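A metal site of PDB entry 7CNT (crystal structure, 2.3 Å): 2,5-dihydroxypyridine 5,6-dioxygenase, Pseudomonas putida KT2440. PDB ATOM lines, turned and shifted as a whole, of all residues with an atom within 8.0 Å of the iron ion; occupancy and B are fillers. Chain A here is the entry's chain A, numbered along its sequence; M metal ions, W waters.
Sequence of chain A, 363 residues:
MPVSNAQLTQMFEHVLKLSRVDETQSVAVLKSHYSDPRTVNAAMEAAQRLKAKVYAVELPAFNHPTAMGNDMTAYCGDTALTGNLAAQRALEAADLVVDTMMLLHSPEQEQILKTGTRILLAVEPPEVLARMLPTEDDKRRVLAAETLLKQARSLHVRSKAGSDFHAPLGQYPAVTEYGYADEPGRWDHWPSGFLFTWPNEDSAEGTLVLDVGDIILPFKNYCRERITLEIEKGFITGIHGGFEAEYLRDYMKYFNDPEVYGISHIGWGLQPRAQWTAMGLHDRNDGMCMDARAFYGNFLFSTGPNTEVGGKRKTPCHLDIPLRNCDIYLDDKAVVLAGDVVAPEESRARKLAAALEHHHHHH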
ATOM      1  N   THR A  73     -21.665  29.193  17.084  1.00  0.00           N
ATOM      2  CA  THR A  73     -21.644  28.956  18.529  1.00  0.00           C
ATOM      3  C   THR A  73     -21.019  30.139  19.282  1.00  0.00           C
ATOM      4  O   THR A  73     -21.224  30.284  20.483  1.00  0.00           O
ATOM      5  CB  THR A  73     -20.875  27.654  18.868  1.00  0.00           C
ATOM      6  OG1 THR A  73     -19.474  27.821  18.623  1.00  0.00           O
ATOM      7  CG2 THR A  73     -21.423  26.476  18.051  1.00  0.00           C
ATOM      8  N   CYS A  76     -24.670  33.154  20.903  1.00  0.00           N
ATOM      9  CA  CYS A  76     -25.911  32.459  21.202  1.00  0.00           C
ATOM     10  C   CYS A  76     -26.988  33.410  21.699  1.00  0.00           C
ATOM     11  O   CYS A  76     -27.354  33.364  22.882  1.00  0.00           O
ATOM     12  CB  CYS A  76     -25.678  31.385  22.264  1.00  0.00           C
ATOM     13  SG  CYS A  76     -24.390  30.191  21.844  1.00  0.00           S
ATOM     14  N   HIS A 105     -29.405  26.978  20.779  1.00  0.00           N
ATOM     15  CA  HIS A 105     -30.312  26.539  21.798  1.00  0.00           C
ATOM     16  C   HIS A 105     -31.070  27.770  22.260  1.00  0.00           C
ATOM     17  O   HIS A 105     -30.477  28.822  22.431  1.00  0.00           O
ATOM     18  CB  HIS A 105     -29.524  25.837  22.876  1.00  0.00           C
ATOM     19  CG  HIS A 105     -28.709  24.709  22.344  1.00  0.00           C
ATOM     20  ND1 HIS A 105     -29.193  23.429  22.235  1.00  0.00           N
ATOM     21  CD2 HIS A 105     -27.460  24.692  21.804  1.00  0.00           C
ATOM     22  CE1 HIS A 105     -28.264  22.648  21.699  1.00  0.00           C
ATOM     23  NE2 HIS A 105     -27.206  23.394  21.422  1.00  0.00           N
ATOM     24  N   PHE A 196     -22.360  15.880  29.763  1.00  0.00           N
ATOM     25  CA  PHE A 196     -22.150  16.992  30.601  1.00  0.00           C
ATOM     26  C   PHE A 196     -23.405  17.277  31.448  1.00  0.00           C
ATOM     27  O   PHE A 196     -24.550  16.850  31.126  1.00  0.00           O
ATOM     28  CB  PHE A 196     -21.798  18.233  29.784  1.00  0.00           C
ATOM     29  CG  PHE A 196     -22.785  18.577  28.708  1.00  0.00           C
ATOM     30  CD1 PHE A 196     -22.658  18.060  27.443  1.00  0.00           C
ATOM     31  CD2 PHE A 196     -23.799  19.455  28.943  1.00  0.00           C
ATOM     32  CE1 PHE A 196     -23.528  18.417  26.430  1.00  0.00           C
ATOM     33  CE2 PHE A 196     -24.705  19.792  27.949  1.00  0.00           C
ATOM     34  CZ  PHE A 196     -24.573  19.282  26.689  1.00  0.00           C
ATOM     35  N   TRP A 198     -24.504  20.717  34.442  1.00  0.00           N
ATOM     36  CA  TRP A 198     -24.201  22.088  34.782  1.00  0.00           C
ATOM     37  C   TRP A 198     -24.024  22.028  36.254  1.00  0.00           C
ATOM     38  O   TRP A 198     -24.545  21.089  36.860  1.00  0.00           O
ATOM     39  CB  TRP A 198     -25.385  23.021  34.511  1.00  0.00           C
ATOM     40  CG  TRP A 198     -25.664  23.288  33.096  1.00  0.00           C
ATOM     41  CD1 TRP A 198     -25.455  24.457  32.424  1.00  0.00           C
ATOM     42  CD2 TRP A 198     -26.272  22.387  32.159  1.00  0.00           C
ATOM     43  NE1 TRP A 198     -25.877  24.339  31.120  1.00  0.00           N
ATOM     44  CE2 TRP A 198     -26.374  23.074  30.929  1.00  0.00           C
ATOM     45  CE3 TRP A 198     -26.727  21.065  32.231  1.00  0.00           C
ATOM     46  CZ2 TRP A 198     -26.929  22.483  29.778  1.00  0.00           C
ATOM     47  CZ3 TRP A 198     -27.269  20.469  31.078  1.00  0.00           C
ATOM     48  CH2 TRP A 198     -27.357  21.189  29.866  1.00  0.00           C
ATOM     49  N   LEU A 217     -12.536  27.151  22.125  1.00  0.00           N
ATOM     50  CA  LEU A 217     -13.459  27.270  21.051  1.00  0.00           C
ATOM     51  C   LEU A 217     -14.340  28.497  21.373  1.00  0.00           C
ATOM     52  O   LEU A 217     -14.772  28.702  22.527  1.00  0.00           O
ATOM     53  CB  LEU A 217     -14.230  25.953  20.917  1.00  0.00           C
ATOM     54  CG  LEU A 217     -13.370  24.689  20.654  1.00  0.00           C
ATOM     55  CD1 LEU A 217     -14.255  23.457  20.518  1.00  0.00           C
ATOM     56  CD2 LEU A 217     -12.504  24.811  19.403  1.00  0.00           C
ATOM     57  N   SER A 264     -20.871  27.323  32.656  1.00  0.00           N
ATOM     58  CA  SER A 264     -22.074  26.643  32.281  1.00  0.00           C
ATOM     59  C   SER A 264     -21.757  25.143  32.206  1.00  0.00           C
ATOM     60  O   SER A 264     -21.328  24.551  33.181  1.00  0.00           O
ATOM     61  CB  SER A 264     -22.637  27.257  31.002  1.00  0.00           C
ATOM     62  OG  SER A 264     -21.697  27.167  29.981  1.00  0.00           O
ATOM     63  N   HIS A 265     -21.925  24.486  31.079  1.00  0.00           N
ATOM     64  CA  HIS A 265     -21.810  23.062  31.168  1.00  0.00           C
ATOM     65  C   HIS A 265     -20.382  22.597  31.428  1.00  0.00           C
ATOM     66  O   HIS A 265     -19.378  23.287  31.117  1.00  0.00           O
ATOM     67  CB  HIS A 265     -22.529  22.324  30.029  1.00  0.00           C
ATOM     68  CG  HIS A 265     -22.046  22.659  28.665  1.00  0.00           C
ATOM     69  ND1 HIS A 265     -20.812  22.253  28.194  1.00  0.00           N
ATOM     70  CD2 HIS A 265     -22.661  23.297  27.638  1.00  0.00           C
ATOM     71  CE1 HIS A 265     -20.680  22.646  26.941  1.00  0.00           C
ATOM     72  NE2 HIS A 265     -21.783  23.280  26.578  1.00  0.00           N
ATOM     73  N   ILE A 266     -20.329  21.429  32.079  1.00  0.00           N
ATOM     74  CA  ILE A 266     -19.117  20.763  32.505  1.00  0.00           C
ATOM     75  C   ILE A 266     -19.294  19.269  32.244  1.00  0.00           C
ATOM     76  O   ILE A 266     -20.385  18.723  32.345  1.00  0.00           O
ATOM     77  CB  ILE A 266     -18.841  20.970  34.016  1.00  0.00           C
ATOM     78  CG1 ILE A 266     -20.073  20.609  34.861  1.00  0.00           C
ATOM     79  CG2 ILE A 266     -18.486  22.406  34.290  1.00  0.00           C
ATOM     80  CD1 ILE A 266     -19.902  20.851  36.344  1.00  0.00           C
ATOM     81  N   ARG A 293     -14.262  18.958  21.095  1.00  0.00           N
ATOM     82  CA  ARG A 293     -15.265  18.857  22.154  1.00  0.00           C
ATOM     83  C   ARG A 293     -15.434  17.452  22.717  1.00  0.00           C
ATOM     84  O   ARG A 293     -15.834  17.289  23.890  1.00  0.00           O
ATOM     85  CB  ARG A 293     -16.618  19.339  21.659  1.00  0.00           C
ATOM     86  CG  ARG A 293     -16.753  20.835  21.631  1.00  0.00           C
ATOM     87  CD  ARG A 293     -18.200  21.215  21.340  1.00  0.00           C
ATOM     88  NE  ARG A 293     -18.248  22.638  21.118  1.00  0.00           N
ATOM     89  CZ  ARG A 293     -17.835  23.247  20.011  1.00  0.00           C
ATOM     90  NH1 ARG A 293     -17.363  22.530  18.993  1.00  0.00           N
ATOM     91  NH2 ARG A 293     -17.900  24.573  19.929  1.00  0.00           N
ATOM     92  N   LEU A 300     -14.316  19.119  29.534  1.00  0.00           N
ATOM     93  CA  LEU A 300     -14.814  20.166  28.672  1.00  0.00           C
ATOM     94  C   LEU A 300     -15.628  21.043  29.511  1.00  0.00           C
ATOM     95  O   LEU A 300     -16.552  20.562  30.191  1.00  0.00           O
ATOM     96  CB  LEU A 300     -15.779  19.605  27.597  1.00  0.00           C
ATOM     97  CG  LEU A 300     -16.483  20.689  26.733  1.00  0.00           C
ATOM     98  CD1 LEU A 300     -15.435  21.468  25.893  1.00  0.00           C
ATOM     99  CD2 LEU A 300     -17.538  20.162  25.814  1.00  0.00           C
ATOM    100  N   PHE A 301     -15.382  22.324  29.451  1.00  0.00           N
ATOM    101  CA  PHE A 301     -16.281  23.171  30.170  1.00  0.00           C
ATOM    102  C   PHE A 301     -16.590  24.349  29.304  1.00  0.00           C
ATOM    103  O   PHE A 301     -15.928  24.552  28.317  1.00  0.00           O
ATOM    104  CB  PHE A 301     -15.701  23.569  31.533  1.00  0.00           C
ATOM    105  CG  PHE A 301     -14.598  24.545  31.464  1.00  0.00           C
ATOM    106  CD1 PHE A 301     -13.299  24.114  31.226  1.00  0.00           C
ATOM    107  CD2 PHE A 301     -14.840  25.897  31.594  1.00  0.00           C
ATOM    108  CE1 PHE A 301     -12.251  25.027  31.136  1.00  0.00           C
ATOM    109  CE2 PHE A 301     -13.783  26.806  31.526  1.00  0.00           C
ATOM    110  CZ  PHE A 301     -12.499  26.372  31.301  1.00  0.00           C
ATOM    111  N   SER A 302     -17.603  25.091  29.692  1.00  0.00           N
ATOM    112  CA  SER A 302     -18.139  26.115  28.832  1.00  0.00           C
ATOM    113  C   SER A 302     -18.450  27.288  29.665  1.00  0.00           C
ATOM    114  O   SER A 302     -18.505  27.190  30.882  1.00  0.00           O
ATOM    115  CB  SER A 302     -19.413  25.593  28.150  1.00  0.00           C
ATOM    116  OG  SER A 302     -19.978  26.569  27.310  1.00  0.00           O
ATOM    117  N   THR A 303     -18.698  28.417  29.011  1.00  0.00           N
ATOM    118  CA  THR A 303     -19.011  29.683  29.685  1.00  0.00           C
ATOM    119  C   THR A 303     -20.162  30.376  28.996  1.00  0.00           C
ATOM    120  O   THR A 303     -20.458  30.048  27.861  1.00  0.00           O
ATOM    121  CB  THR A 303     -17.809  30.654  29.574  1.00  0.00           C
ATOM    122  OG1 THR A 303     -17.481  30.872  28.207  1.00  0.00           O
ATOM    123  CG2 THR A 303     -16.558  30.091  30.284  1.00  0.00           C
ATOM    124  N   GLY A 304     -20.759  31.353  29.654  1.00  0.00           N
ATOM    125  CA  GLY A 304     -21.824  32.140  29.038  1.00  0.00           C
ATOM    126  C   GLY A 304     -23.233  31.659  29.386  1.00  0.00           C
ATOM    127  O   GLY A 304     -23.558  31.497  30.549  1.00  0.00           O
ATOM    128  N   PRO A 305     -24.085  31.427  28.360  1.00  0.00           N
ATOM    129  CA  PRO A 305     -25.512  31.174  28.581  1.00  0.00           C
ATOM    130  C   PRO A 305     -25.859  29.798  29.138  1.00  0.00           C
ATOM    131  O   PRO A 305     -25.407  28.743  28.637  1.00  0.00           O
ATOM    132  CB  PRO A 305     -26.116  31.326  27.176  1.00  0.00           C
ATOM    133  CG  PRO A 305     -25.020  30.912  26.264  1.00  0.00           C
ATOM    134  CD  PRO A 305     -23.746  31.375  26.921  1.00  0.00           C
ATOM    135  N   GLU A 308     -30.703  27.478  28.466  1.00  0.00           N
ATOM    136  CA  GLU A 308     -31.185  26.185  27.971  1.00  0.00           C
ATOM    137  C   GLU A 308     -31.817  25.344  29.065  1.00  0.00           C
ATOM    138  O   GLU A 308     -32.757  24.607  28.791  1.00  0.00           O
ATOM    139  CB  GLU A 308     -30.049  25.376  27.354  1.00  0.00           C
ATOM    140  CG  GLU A 308     -29.291  26.075  26.224  1.00  0.00           C
ATOM    141  CD  GLU A 308     -27.810  26.330  26.516  1.00  0.00           C
ATOM    142  OE1 GLU A 308     -27.245  27.349  26.038  1.00  0.00           O
ATOM    143  OE2 GLU A 308     -27.196  25.494  27.226  1.00  0.00           O
ATOM    144  N   HIS A 318     -20.224  32.785  24.116  1.00  0.00           N
ATOM    145  CA  HIS A 318     -20.158  31.394  24.461  1.00  0.00           C
ATOM    146  C   HIS A 318     -18.774  30.843  24.091  1.00  0.00           C
ATOM    147  O   HIS A 318     -18.344  30.970  22.957  1.00  0.00           O
ATOM    148  CB  HIS A 318     -21.254  30.685  23.675  1.00  0.00           C
ATOM    149  CG  HIS A 318     -21.248  29.192  23.815  1.00  0.00           C
ATOM    150  ND1 HIS A 318     -20.716  28.366  22.856  1.00  0.00           N
ATOM    151  CD2 HIS A 318     -21.744  28.392  24.780  1.00  0.00           C
ATOM    152  CE1 HIS A 318     -20.863  27.108  23.233  1.00  0.00           C
ATOM    153  NE2 HIS A 318     -21.480  27.103  24.396  1.00  0.00           N
ATOM    154  N   LEU A 319     -18.091  30.244  25.064  1.00  0.00           N
ATOM    155  CA  LEU A 319     -16.814  29.565  24.867  1.00  0.00           C
ATOM    156  C   LEU A 319     -16.919  28.105  25.243  1.00  0.00           C
ATOM    157  O   LEU A 319     -17.616  27.749  26.201  1.00  0.00           O
ATOM    158  CB  LEU A 319     -15.735  30.161  25.776  1.00  0.00           C
ATOM    159  CG  LEU A 319     -15.568  31.684  25.801  1.00  0.00           C
ATOM    160  CD1 LEU A 319     -14.423  31.982  26.690  1.00  0.00           C
ATOM    161  CD2 LEU A 319     -15.271  32.189  24.404  1.00  0.00           C
ATOM    162  N   ASP A 320     -16.165  27.267  24.550  1.00  0.00           N
ATOM    163  CA  ASP A 320     -16.082  25.857  24.894  1.00  0.00           C
ATOM    164  C   ASP A 320     -14.608  25.539  25.036  1.00  0.00           C
ATOM    165  O   ASP A 320     -13.834  25.872  24.168  1.00  0.00           O
ATOM    166  CB  ASP A 320     -16.679  25.007  23.776  1.00  0.00           C
ATOM    167  CG  ASP A 320     -18.165  24.677  23.983  1.00  0.00           C
ATOM    168  OD1 ASP A 320     -18.690  24.825  25.091  1.00  0.00           O
ATOM    169  OD2 ASP A 320     -18.802  24.217  23.026  1.00  0.00           O
ATOM    170  N   ILE A 321     -14.221  24.910  26.149  1.00  0.00           N
ATOM    171  CA  ILE A 321     -12.812  24.733  26.476  1.00  0.00           C
ATOM    172  C   ILE A 321     -12.449  23.291  26.928  1.00  0.00           C
ATOM    173  O   ILE A 321     -12.730  22.904  28.044  1.00  0.00           O
ATOM    174  CB  ILE A 321     -12.394  25.733  27.550  1.00  0.00           C
ATOM    175  CG1 ILE A 321     -12.517  27.153  27.023  1.00  0.00           C
ATOM    176  CG2 ILE A 321     -10.943  25.496  27.952  1.00  0.00           C
ATOM    177  CD1 ILE A 321     -12.332  28.221  28.085  1.00  0.00           C
HETATM  178 FE    FE M   1     -21.075  25.505  25.540  1.00  0.00          FE
HETATM  179  O   HOH W   1     -22.596  23.709  23.559  1.00  0.00           O
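ND1 of His 318 is in hydrogen-bond range of O of Thr 73 (3.1 Å).
The side-chain hydroxyl (OG) of Ser 302 sits close to the backbone carbonyl oxygen (O) of Leu 319, 2.9 Å away.
O of Ser 302 lies within hydrogen-bond range of N of Ser 264, 3.0 Å away.
The side-chain carboxylate of Asp 320 lies within salt-bridge range of the guanidinium group of Arg 293 (2.5 Å).
The backbone NH of Leu 217 sits at hydrogen-bond distance from the backbone carbonyl oxygen of Asp 320.
Within 4 Å of the iron ion: His 265, Ser 302, His 318 and Asp 320.
NE2 of His 318 binds the iron ion, 2.0 Å away.
The side-chain hydroxyl (OG) of Ser 302 is bound to the iron ion.
OD1 of Asp 320 is bound to the iron ion (2.5 Å).
The iron ion is bound by NE2 of His 265, at 2.6 Å.
The iron ion has four donor atoms within binding distance.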
